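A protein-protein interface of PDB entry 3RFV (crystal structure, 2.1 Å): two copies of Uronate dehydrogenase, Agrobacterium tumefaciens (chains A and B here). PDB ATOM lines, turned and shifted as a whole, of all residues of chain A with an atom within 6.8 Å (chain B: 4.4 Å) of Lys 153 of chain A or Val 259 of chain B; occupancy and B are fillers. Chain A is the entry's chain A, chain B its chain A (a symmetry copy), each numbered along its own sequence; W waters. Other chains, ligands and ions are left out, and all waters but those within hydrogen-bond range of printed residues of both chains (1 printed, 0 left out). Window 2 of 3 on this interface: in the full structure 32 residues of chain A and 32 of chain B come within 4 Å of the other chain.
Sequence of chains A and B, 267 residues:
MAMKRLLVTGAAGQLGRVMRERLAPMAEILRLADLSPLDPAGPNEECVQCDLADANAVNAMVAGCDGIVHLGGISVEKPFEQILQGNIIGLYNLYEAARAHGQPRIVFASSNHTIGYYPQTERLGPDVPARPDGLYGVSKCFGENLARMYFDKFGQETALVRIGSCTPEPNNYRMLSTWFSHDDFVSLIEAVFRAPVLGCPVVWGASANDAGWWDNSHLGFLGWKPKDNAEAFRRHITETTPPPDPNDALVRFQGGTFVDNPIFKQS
The side-chain hydroxyl of Tyr 117 of chain B is in hydrogen-bond range of the backbone carbonyl oxygen of Val 259 of chain B (3.2 Å). The guanidinium group (NH2) of Arg 148 of chain A is in salt-bridge range of the side-chain carboxylate (OD1) of Asp 152 of chain A (2.9 Å).
NZ of Lys 153 of chain A lies within hydrogen-bond range of O of Asp 133 of chain B (2.9 Å). The side-chain amino group (NZ) of Lys 153 of chain A lies within hydrogen-bond range of the backbone carbonyl oxygen (O) of Asn 261 of chain B. OH of Tyr 117 of chain B lies close to NZ of Lys 153 of chain A (3.3 Å). The backbone carbonyl oxygen (O) of Phe 258 of chain B lies within hydrogen-bond range of the side-chain amino group (NZ) of Lys 153 of chain A (3.4 Å). O of Val 259 of chain B is in hydrogen-bond range of NZ of Lys 153 of chain A.
Water W1 bridges the backbone carbonyl oxygen of Asn 261 of chain B and the side-chain amino group of Lys 153 of chain A.
No position is printed for both chains. Of the 8 pairs that touch across the chains among the printed residues, none has its exchanged pair printed and touching as well.
C of Asp 133 of chain B touches CG of Met 149 of chain A (3.9 Å). CG of Met 149 of chain A touches N of Gly 134 of chain B, at 3.5 Å. CD2 of Tyr 117 of chain B touches CB of Asp 152 of chain A, 3.5 Å away.
Arg 148 of chain A touches none of the printed residues of chain B. Tyr 150 of chain A touches none of the printed residues of chain B. Of the printed residues of chain B, Asp 152 of chain A touches Tyr 117 (3.5 Å). Of the printed residues of chain B, Lys 153 of chain A touches Tyr 117, Asp 133, Phe 258, Val 259 and Asn 261. Of the printed residues of chain A, Tyr 117 of chain B touches Asp 152 (3.5 Å) and Lys 153 (3.2 Å). Of the printed residues of chain A, Gly 134 of chain B touches Met 149. Of the printed residues of chain A, Phe 258 of chain B touches Lys 153. Val 259 of chain B touches one residue of chain A.
Printed residues of chain A that touch a printed residue of chain B: Met 149, Asp 152 and Lys 153. Along chain A the printed residues that touch a printed residue of chain B span positions 149 to 153. Printed residues of chain B that touch a printed residue of chain A: Tyr 117, Asp 133, Gly 134, Phe 258, Val 259 and Asn 261. Hydrophobic or aromatic side chains of chain B that line the printed part of chain A: Tyr 117. Among the printed residues, 8 pairs touch across the chains.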
ATOM      1  N   GLN A 103     -41.156 -37.961  -3.239  1.00  0.00           N
ATOM      2  CA  GLN A 103     -39.801 -38.513  -3.346  1.00  0.00           C
ATOM      3  C   GLN A 103     -39.755 -40.022  -3.143  1.00  0.00           C
ATOM      4  O   GLN A 103     -39.019 -40.522  -2.295  1.00  0.00           O
ATOM      5  CB  GLN A 103     -38.853 -37.813  -2.359  1.00  0.00           C
ATOM      6  CG  GLN A 103     -38.529 -36.400  -2.780  1.00  0.00           C
ATOM      7  CD  GLN A 103     -37.701 -35.619  -1.766  1.00  0.00           C
ATOM      8  OE1 GLN A 103     -37.508 -34.417  -1.925  1.00  0.00           O
ATOM      9  NE2 GLN A 103     -37.207 -36.293  -0.729  1.00  0.00           N
ATOM     10  N   ARG A 148     -27.254 -37.678  -6.903  1.00  0.00           N
ATOM     11  CA  ARG A 148     -26.509 -37.290  -5.705  1.00  0.00           C
ATOM     12  C   ARG A 148     -26.898 -35.885  -5.243  1.00  0.00           C
ATOM     13  O   ARG A 148     -27.089 -35.656  -4.053  1.00  0.00           O
ATOM     14  CB  ARG A 148     -24.993 -37.386  -5.911  1.00  0.00           C
ATOM     15  CG  ARG A 148     -24.171 -36.957  -4.672  1.00  0.00           C
ATOM     16  CD  ARG A 148     -24.330 -37.935  -3.502  1.00  0.00           C
ATOM     17  NE  ARG A 148     -24.189 -37.279  -2.196  1.00  0.00           N
ATOM     18  CZ  ARG A 148     -23.838 -37.903  -1.070  1.00  0.00           C
ATOM     19  NH1 ARG A 148     -23.547 -39.195  -1.079  1.00  0.00           N
ATOM     20  NH2 ARG A 148     -23.757 -37.227   0.070  1.00  0.00           N
ATOM     21  N   MET A 149     -27.001 -34.952  -6.186  1.00  0.00           N
ATOM     22  CA  MET A 149     -27.418 -33.586  -5.877  1.00  0.00           C
ATOM     23  C   MET A 149     -28.812 -33.564  -5.236  1.00  0.00           C
ATOM     24  O   MET A 149     -29.024 -32.874  -4.232  1.00  0.00           O
ATOM     25  CB  MET A 149     -27.360 -32.696  -7.132  1.00  0.00           C
ATOM     26  CG  MET A 149     -27.681 -31.218  -6.890  1.00  0.00           C
ATOM     27  SD  MET A 149     -29.467 -30.895  -7.006  1.00  0.00           S
ATOM     28  CE  MET A 149     -29.711 -31.008  -8.792  1.00  0.00           C
ATOM     29  N   TYR A 150     -29.749 -34.325  -5.801  1.00  0.00           N
ATOM     30  CA  TYR A 150     -31.089 -34.430  -5.227  1.00  0.00           C
ATOM     31  C   TYR A 150     -31.079 -35.016  -3.826  1.00  0.00           C
ATOM     32  O   TYR A 150     -31.888 -34.611  -2.975  1.00  0.00           O
ATOM     33  CB  TYR A 150     -32.063 -35.197  -6.144  1.00  0.00           C
ATOM     34  CG  TYR A 150     -32.649 -34.302  -7.211  1.00  0.00           C
ATOM     35  CD1 TYR A 150     -33.901 -33.714  -7.051  1.00  0.00           C
ATOM     36  CD2 TYR A 150     -31.933 -34.017  -8.366  1.00  0.00           C
ATOM     37  CE1 TYR A 150     -34.429 -32.880  -8.029  1.00  0.00           C
ATOM     38  CE2 TYR A 150     -32.445 -33.196  -9.342  1.00  0.00           C
ATOM     39  CZ  TYR A 150     -33.697 -32.625  -9.171  1.00  0.00           C
ATOM     40  OH  TYR A 150     -34.187 -31.801 -10.157  1.00  0.00           O
ATOM     41  N   PHE A 151     -30.171 -35.956  -3.573  1.00  0.00           N
ATOM     42  CA  PHE A 151     -30.047 -36.502  -2.229  1.00  0.00           C
ATOM     43  C   PHE A 151     -29.534 -35.456  -1.233  1.00  0.00           C
ATOM     44  O   PHE A 151     -30.112 -35.277  -0.162  1.00  0.00           O
ATOM     45  CB  PHE A 151     -29.149 -37.738  -2.184  1.00  0.00           C
ATOM     46  CG  PHE A 151     -28.808 -38.171  -0.778  1.00  0.00           C
ATOM     47  CD1 PHE A 151     -29.778 -38.725   0.042  1.00  0.00           C
ATOM     48  CD2 PHE A 151     -27.528 -37.998  -0.277  1.00  0.00           C
ATOM     49  CE1 PHE A 151     -29.478 -39.109   1.339  1.00  0.00           C
ATOM     50  CE2 PHE A 151     -27.211 -38.383   1.025  1.00  0.00           C
ATOM     51  CZ  PHE A 151     -28.191 -38.941   1.833  1.00  0.00           C
ATOM     52  N   ASP A 152     -28.439 -34.785  -1.584  1.00  0.00           N
ATOM     53  CA  ASP A 152     -27.865 -33.762  -0.716  1.00  0.00           C
ATOM     54  C   ASP A 152     -28.804 -32.567  -0.530  1.00  0.00           C
ATOM     55  O   ASP A 152     -28.868 -31.988   0.549  1.00  0.00           O
ATOM     56  CB  ASP A 152     -26.509 -33.284  -1.248  1.00  0.00           C
ATOM     57  CG  ASP A 152     -25.381 -34.260  -0.940  1.00  0.00           C
ATOM     58  OD1 ASP A 152     -25.413 -34.882   0.145  1.00  0.00           O
ATOM     59  OD2 ASP A 152     -24.466 -34.405  -1.785  1.00  0.00           O
ATOM     60  N   LYS A 153     -29.523 -32.202  -1.587  1.00  0.00           N
ATOM     61  CA  LYS A 153     -30.359 -31.011  -1.537  1.00  0.00           C
ATOM     62  C   LYS A 153     -31.741 -31.277  -0.931  1.00  0.00           C
ATOM     63  O   LYS A 153     -32.239 -30.453  -0.182  1.00  0.00           O
ATOM     64  CB  LYS A 153     -30.492 -30.364  -2.922  1.00  0.00           C
ATOM     65  CG  LYS A 153     -31.124 -28.952  -2.898  1.00  0.00           C
ATOM     66  CD  LYS A 153     -31.115 -28.335  -4.299  1.00  0.00           C
ATOM     67  CE  LYS A 153     -29.707 -27.986  -4.750  1.00  0.00           C
ATOM     68  NZ  LYS A 153     -29.139 -26.802  -4.016  1.00  0.00           N
ATOM     69  N   PHE A 154     -32.345 -32.427  -1.236  1.00  0.00           N
ATOM     70  CA  PHE A 154     -33.746 -32.669  -0.878  1.00  0.00           C
ATOM     71  C   PHE A 154     -33.990 -33.945  -0.076  1.00  0.00           C
ATOM     72  O   PHE A 154     -35.098 -34.166   0.412  1.00  0.00           O
ATOM     73  CB  PHE A 154     -34.629 -32.707  -2.135  1.00  0.00           C
ATOM     74  CG  PHE A 154     -34.604 -31.437  -2.931  1.00  0.00           C
ATOM     75  CD1 PHE A 154     -35.223 -30.291  -2.450  1.00  0.00           C
ATOM     76  CD2 PHE A 154     -33.974 -31.391  -4.167  1.00  0.00           C
ATOM     77  CE1 PHE A 154     -35.210 -29.120  -3.188  1.00  0.00           C
ATOM     78  CE2 PHE A 154     -33.951 -30.221  -4.911  1.00  0.00           C
ATOM     79  CZ  PHE A 154     -34.572 -29.082  -4.422  1.00  0.00           C
ATOM     80  N   GLY A 155     -32.971 -34.787   0.048  1.00  0.00           N
ATOM     81  CA  GLY A 155     -33.118 -36.047   0.758  1.00  0.00           C
ATOM     82  C   GLY A 155     -33.641 -37.193  -0.101  1.00  0.00           C
ATOM     83  O   GLY A 155     -33.891 -38.294   0.401  1.00  0.00           O
ATOM     84  N   GLN A 156     -33.822 -36.944  -1.391  1.00  0.00           N
ATOM     85  CA  GLN A 156     -34.253 -38.006  -2.305  1.00  0.00           C
ATOM     86  C   GLN A 156     -33.253 -39.158  -2.244  1.00  0.00           C
ATOM     87  O   GLN A 156     -32.064 -38.945  -2.437  1.00  0.00           O
ATOM     88  CB  GLN A 156     -34.323 -37.476  -3.738  1.00  0.00           C
ATOM     89  CG  GLN A 156     -34.519 -38.574  -4.783  1.00  0.00           C
ATOM     90  CD  GLN A 156     -35.900 -39.193  -4.730  1.00  0.00           C
ATOM     91  OE1 GLN A 156     -36.904 -38.504  -4.926  1.00  0.00           O
ATOM     92  NE2 GLN A 156     -35.964 -40.497  -4.459  1.00  0.00           N
ATOM     93  N   GLY B 116     -19.703 -28.883  -4.113  1.00  0.00           N
ATOM     94  CA  GLY B 116     -20.220 -27.840  -3.244  1.00  0.00           C
ATOM     95  C   GLY B 116     -20.803 -28.313  -1.920  1.00  0.00           C
ATOM     96  O   GLY B 116     -20.823 -27.545  -0.948  1.00  0.00           O
ATOM     97  N   TYR B 117     -21.284 -29.557  -1.871  1.00  0.00           N
ATOM     98  CA  TYR B 117     -21.887 -30.086  -0.641  1.00  0.00           C
ATOM     99  C   TYR B 117     -20.912 -30.615   0.418  1.00  0.00           C
ATOM    100  O   TYR B 117     -21.341 -30.987   1.505  1.00  0.00           O
ATOM    101  CB  TYR B 117     -22.978 -31.130  -0.932  1.00  0.00           C
ATOM    102  CG  TYR B 117     -24.348 -30.504  -1.072  1.00  0.00           C
ATOM    103  CD1 TYR B 117     -25.039 -30.038   0.043  1.00  0.00           C
ATOM    104  CD2 TYR B 117     -24.935 -30.350  -2.324  1.00  0.00           C
ATOM    105  CE1 TYR B 117     -26.293 -29.446  -0.085  1.00  0.00           C
ATOM    106  CE2 TYR B 117     -26.183 -29.779  -2.465  1.00  0.00           C
ATOM    107  CZ  TYR B 117     -26.856 -29.316  -1.345  1.00  0.00           C
ATOM    108  OH  TYR B 117     -28.094 -28.737  -1.503  1.00  0.00           O
ATOM    109  N   ASP B 133     -23.750 -29.110  -6.156  1.00  0.00           N
ATOM    110  CA  ASP B 133     -24.694 -28.388  -5.296  1.00  0.00           C
ATOM    111  C   ASP B 133     -25.901 -27.809  -6.043  1.00  0.00           C
ATOM    112  O   ASP B 133     -26.682 -27.051  -5.470  1.00  0.00           O
ATOM    113  CB  ASP B 133     -23.975 -27.314  -4.464  1.00  0.00           C
ATOM    114  CG  ASP B 133     -23.205 -26.314  -5.315  1.00  0.00           C
ATOM    115  OD1 ASP B 133     -23.594 -26.094  -6.477  1.00  0.00           O
ATOM    116  OD2 ASP B 133     -22.217 -25.731  -4.814  1.00  0.00           O
ATOM    117  N   GLY B 134     -26.057 -28.187  -7.313  1.00  0.00           N
ATOM    118  CA  GLY B 134     -27.218 -27.797  -8.101  1.00  0.00           C
ATOM    119  C   GLY B 134     -27.091 -28.280  -9.541  1.00  0.00           C
ATOM    120  O   GLY B 134     -26.153 -29.009  -9.871  1.00  0.00           O
ATOM    121  N   ALA B 249     -24.550 -20.963   5.118  1.00  0.00           N
ATOM    122  CA  ALA B 249     -23.931 -21.861   4.142  1.00  0.00           C
ATOM    123  C   ALA B 249     -22.563 -21.329   3.723  1.00  0.00           C
ATOM    124  O   ALA B 249     -21.657 -22.095   3.383  1.00  0.00           O
ATOM    125  CB  ALA B 249     -24.830 -22.024   2.934  1.00  0.00           C
ATOM    126  N   PHE B 253     -20.511 -24.894   3.846  1.00  0.00           N
ATOM    127  CA  PHE B 253     -20.391 -25.723   2.651  1.00  0.00           C
ATOM    128  C   PHE B 253     -19.421 -25.114   1.658  1.00  0.00           C
ATOM    129  O   PHE B 253     -19.348 -23.889   1.497  1.00  0.00           O
ATOM    130  CB  PHE B 253     -21.758 -25.925   2.002  1.00  0.00           C
ATOM    131  CG  PHE B 253     -22.729 -26.634   2.889  1.00  0.00           C
ATOM    132  CD1 PHE B 253     -22.692 -28.015   3.007  1.00  0.00           C
ATOM    133  CD2 PHE B 253     -23.653 -25.919   3.641  1.00  0.00           C
ATOM    134  CE1 PHE B 253     -23.578 -28.682   3.847  1.00  0.00           C
ATOM    135  CE2 PHE B 253     -24.548 -26.575   4.476  1.00  0.00           C
ATOM    136  CZ  PHE B 253     -24.508 -27.963   4.580  1.00  0.00           C
ATOM    137  N   GLY B 256     -20.801 -22.823  -0.660  1.00  0.00           N
ATOM    138  CA  GLY B 256     -21.422 -21.652  -0.059  1.00  0.00           C
ATOM    139  C   GLY B 256     -22.926 -21.666  -0.265  1.00  0.00           C
ATOM    140  O   GLY B 256     -23.556 -22.720  -0.144  1.00  0.00           O
ATOM    141  N   THR B 257     -23.502 -20.513  -0.598  1.00  0.00           N
ATOM    142  CA  THR B 257     -24.961 -20.404  -0.697  1.00  0.00           C
ATOM    143  C   THR B 257     -25.592 -21.133  -1.886  1.00  0.00           C
ATOM    144  O   THR B 257     -26.812 -21.263  -1.941  1.00  0.00           O
ATOM    145  CB  THR B 257     -25.438 -18.940  -0.726  1.00  0.00           C
ATOM    146  OG1 THR B 257     -24.845 -18.274  -1.843  1.00  0.00           O
ATOM    147  CG2 THR B 257     -25.063 -18.217   0.584  1.00  0.00           C
ATOM    148  N   PHE B 258     -24.786 -21.621  -2.828  1.00  0.00           N
ATOM    149  CA  PHE B 258     -25.361 -22.461  -3.883  1.00  0.00           C
ATOM    150  C   PHE B 258     -26.151 -23.619  -3.294  1.00  0.00           C
ATOM    151  O   PHE B 258     -27.146 -24.041  -3.884  1.00  0.00           O
ATOM    152  CB  PHE B 258     -24.301 -22.985  -4.872  1.00  0.00           C
ATOM    153  CG  PHE B 258     -23.974 -22.016  -5.996  1.00  0.00           C
ATOM    154  CD1 PHE B 258     -23.993 -22.436  -7.322  1.00  0.00           C
ATOM    155  CD2 PHE B 258     -23.644 -20.696  -5.726  1.00  0.00           C
ATOM    156  CE1 PHE B 258     -23.680 -21.560  -8.356  1.00  0.00           C
ATOM    157  CE2 PHE B 258     -23.334 -19.810  -6.759  1.00  0.00           C
ATOM    158  CZ  PHE B 258     -23.351 -20.247  -8.076  1.00  0.00           C
ATOM    159  N   VAL B 259     -25.737 -24.142  -2.135  1.00  0.00           N
ATOM    160  CA  VAL B 259     -26.497 -25.249  -1.551  1.00  0.00           C
ATOM    161  C   VAL B 259     -27.924 -24.815  -1.221  1.00  0.00           C
ATOM    162  O   VAL B 259     -28.858 -25.638  -1.221  1.00  0.00           O
ATOM    163  CB  VAL B 259     -25.839 -25.863  -0.293  1.00  0.00           C
ATOM    164  CG1 VAL B 259     -24.427 -26.405  -0.614  1.00  0.00           C
ATOM    165  CG2 VAL B 259     -25.808 -24.847   0.855  1.00  0.00           C
ATOM    166  N   ASP B 260     -28.086 -23.519  -0.956  1.00  0.00           N
ATOM    167  CA  ASP B 260     -29.388 -22.952  -0.615  1.00  0.00           C
ATOM    168  C   ASP B 260     -30.278 -22.725  -1.850  1.00  0.00           C
ATOM    169  O   ASP B 260     -31.484 -22.493  -1.719  1.00  0.00           O
ATOM    170  CB  ASP B 260     -29.206 -21.621   0.125  1.00  0.00           C
ATOM    171  CG  ASP B 260     -28.575 -21.789   1.497  1.00  0.00           C
ATOM    172  OD1 ASP B 260     -28.738 -22.861   2.114  1.00  0.00           O
ATOM    173  OD2 ASP B 260     -27.923 -20.833   1.962  1.00  0.00           O
ATOM    174  N   ASN B 261     -29.689 -22.748  -3.043  1.00  0.00           N
ATOM    175  CA  ASN B 261     -30.496 -22.614  -4.263  1.00  0.00           C
ATOM    176  C   ASN B 261     -31.497 -23.749  -4.375  1.00  0.00           C
ATOM    177  O   ASN B 261     -31.147 -24.910  -4.146  1.00  0.00           O
ATOM    178  CB  ASN B 261     -29.631 -22.621  -5.520  1.00  0.00           C
ATOM    179  CG  ASN B 261     -28.835 -21.354  -5.695  1.00  0.00           C
ATOM    180  OD1 ASN B 261     -29.218 -20.284  -5.215  1.00  0.00           O
ATOM    181  ND2 ASN B 261     -27.711 -21.462  -6.397  1.00  0.00           N
HETATM  182  O   HOH W   1     -29.872 -25.627  -7.163  1.00  0.00           O
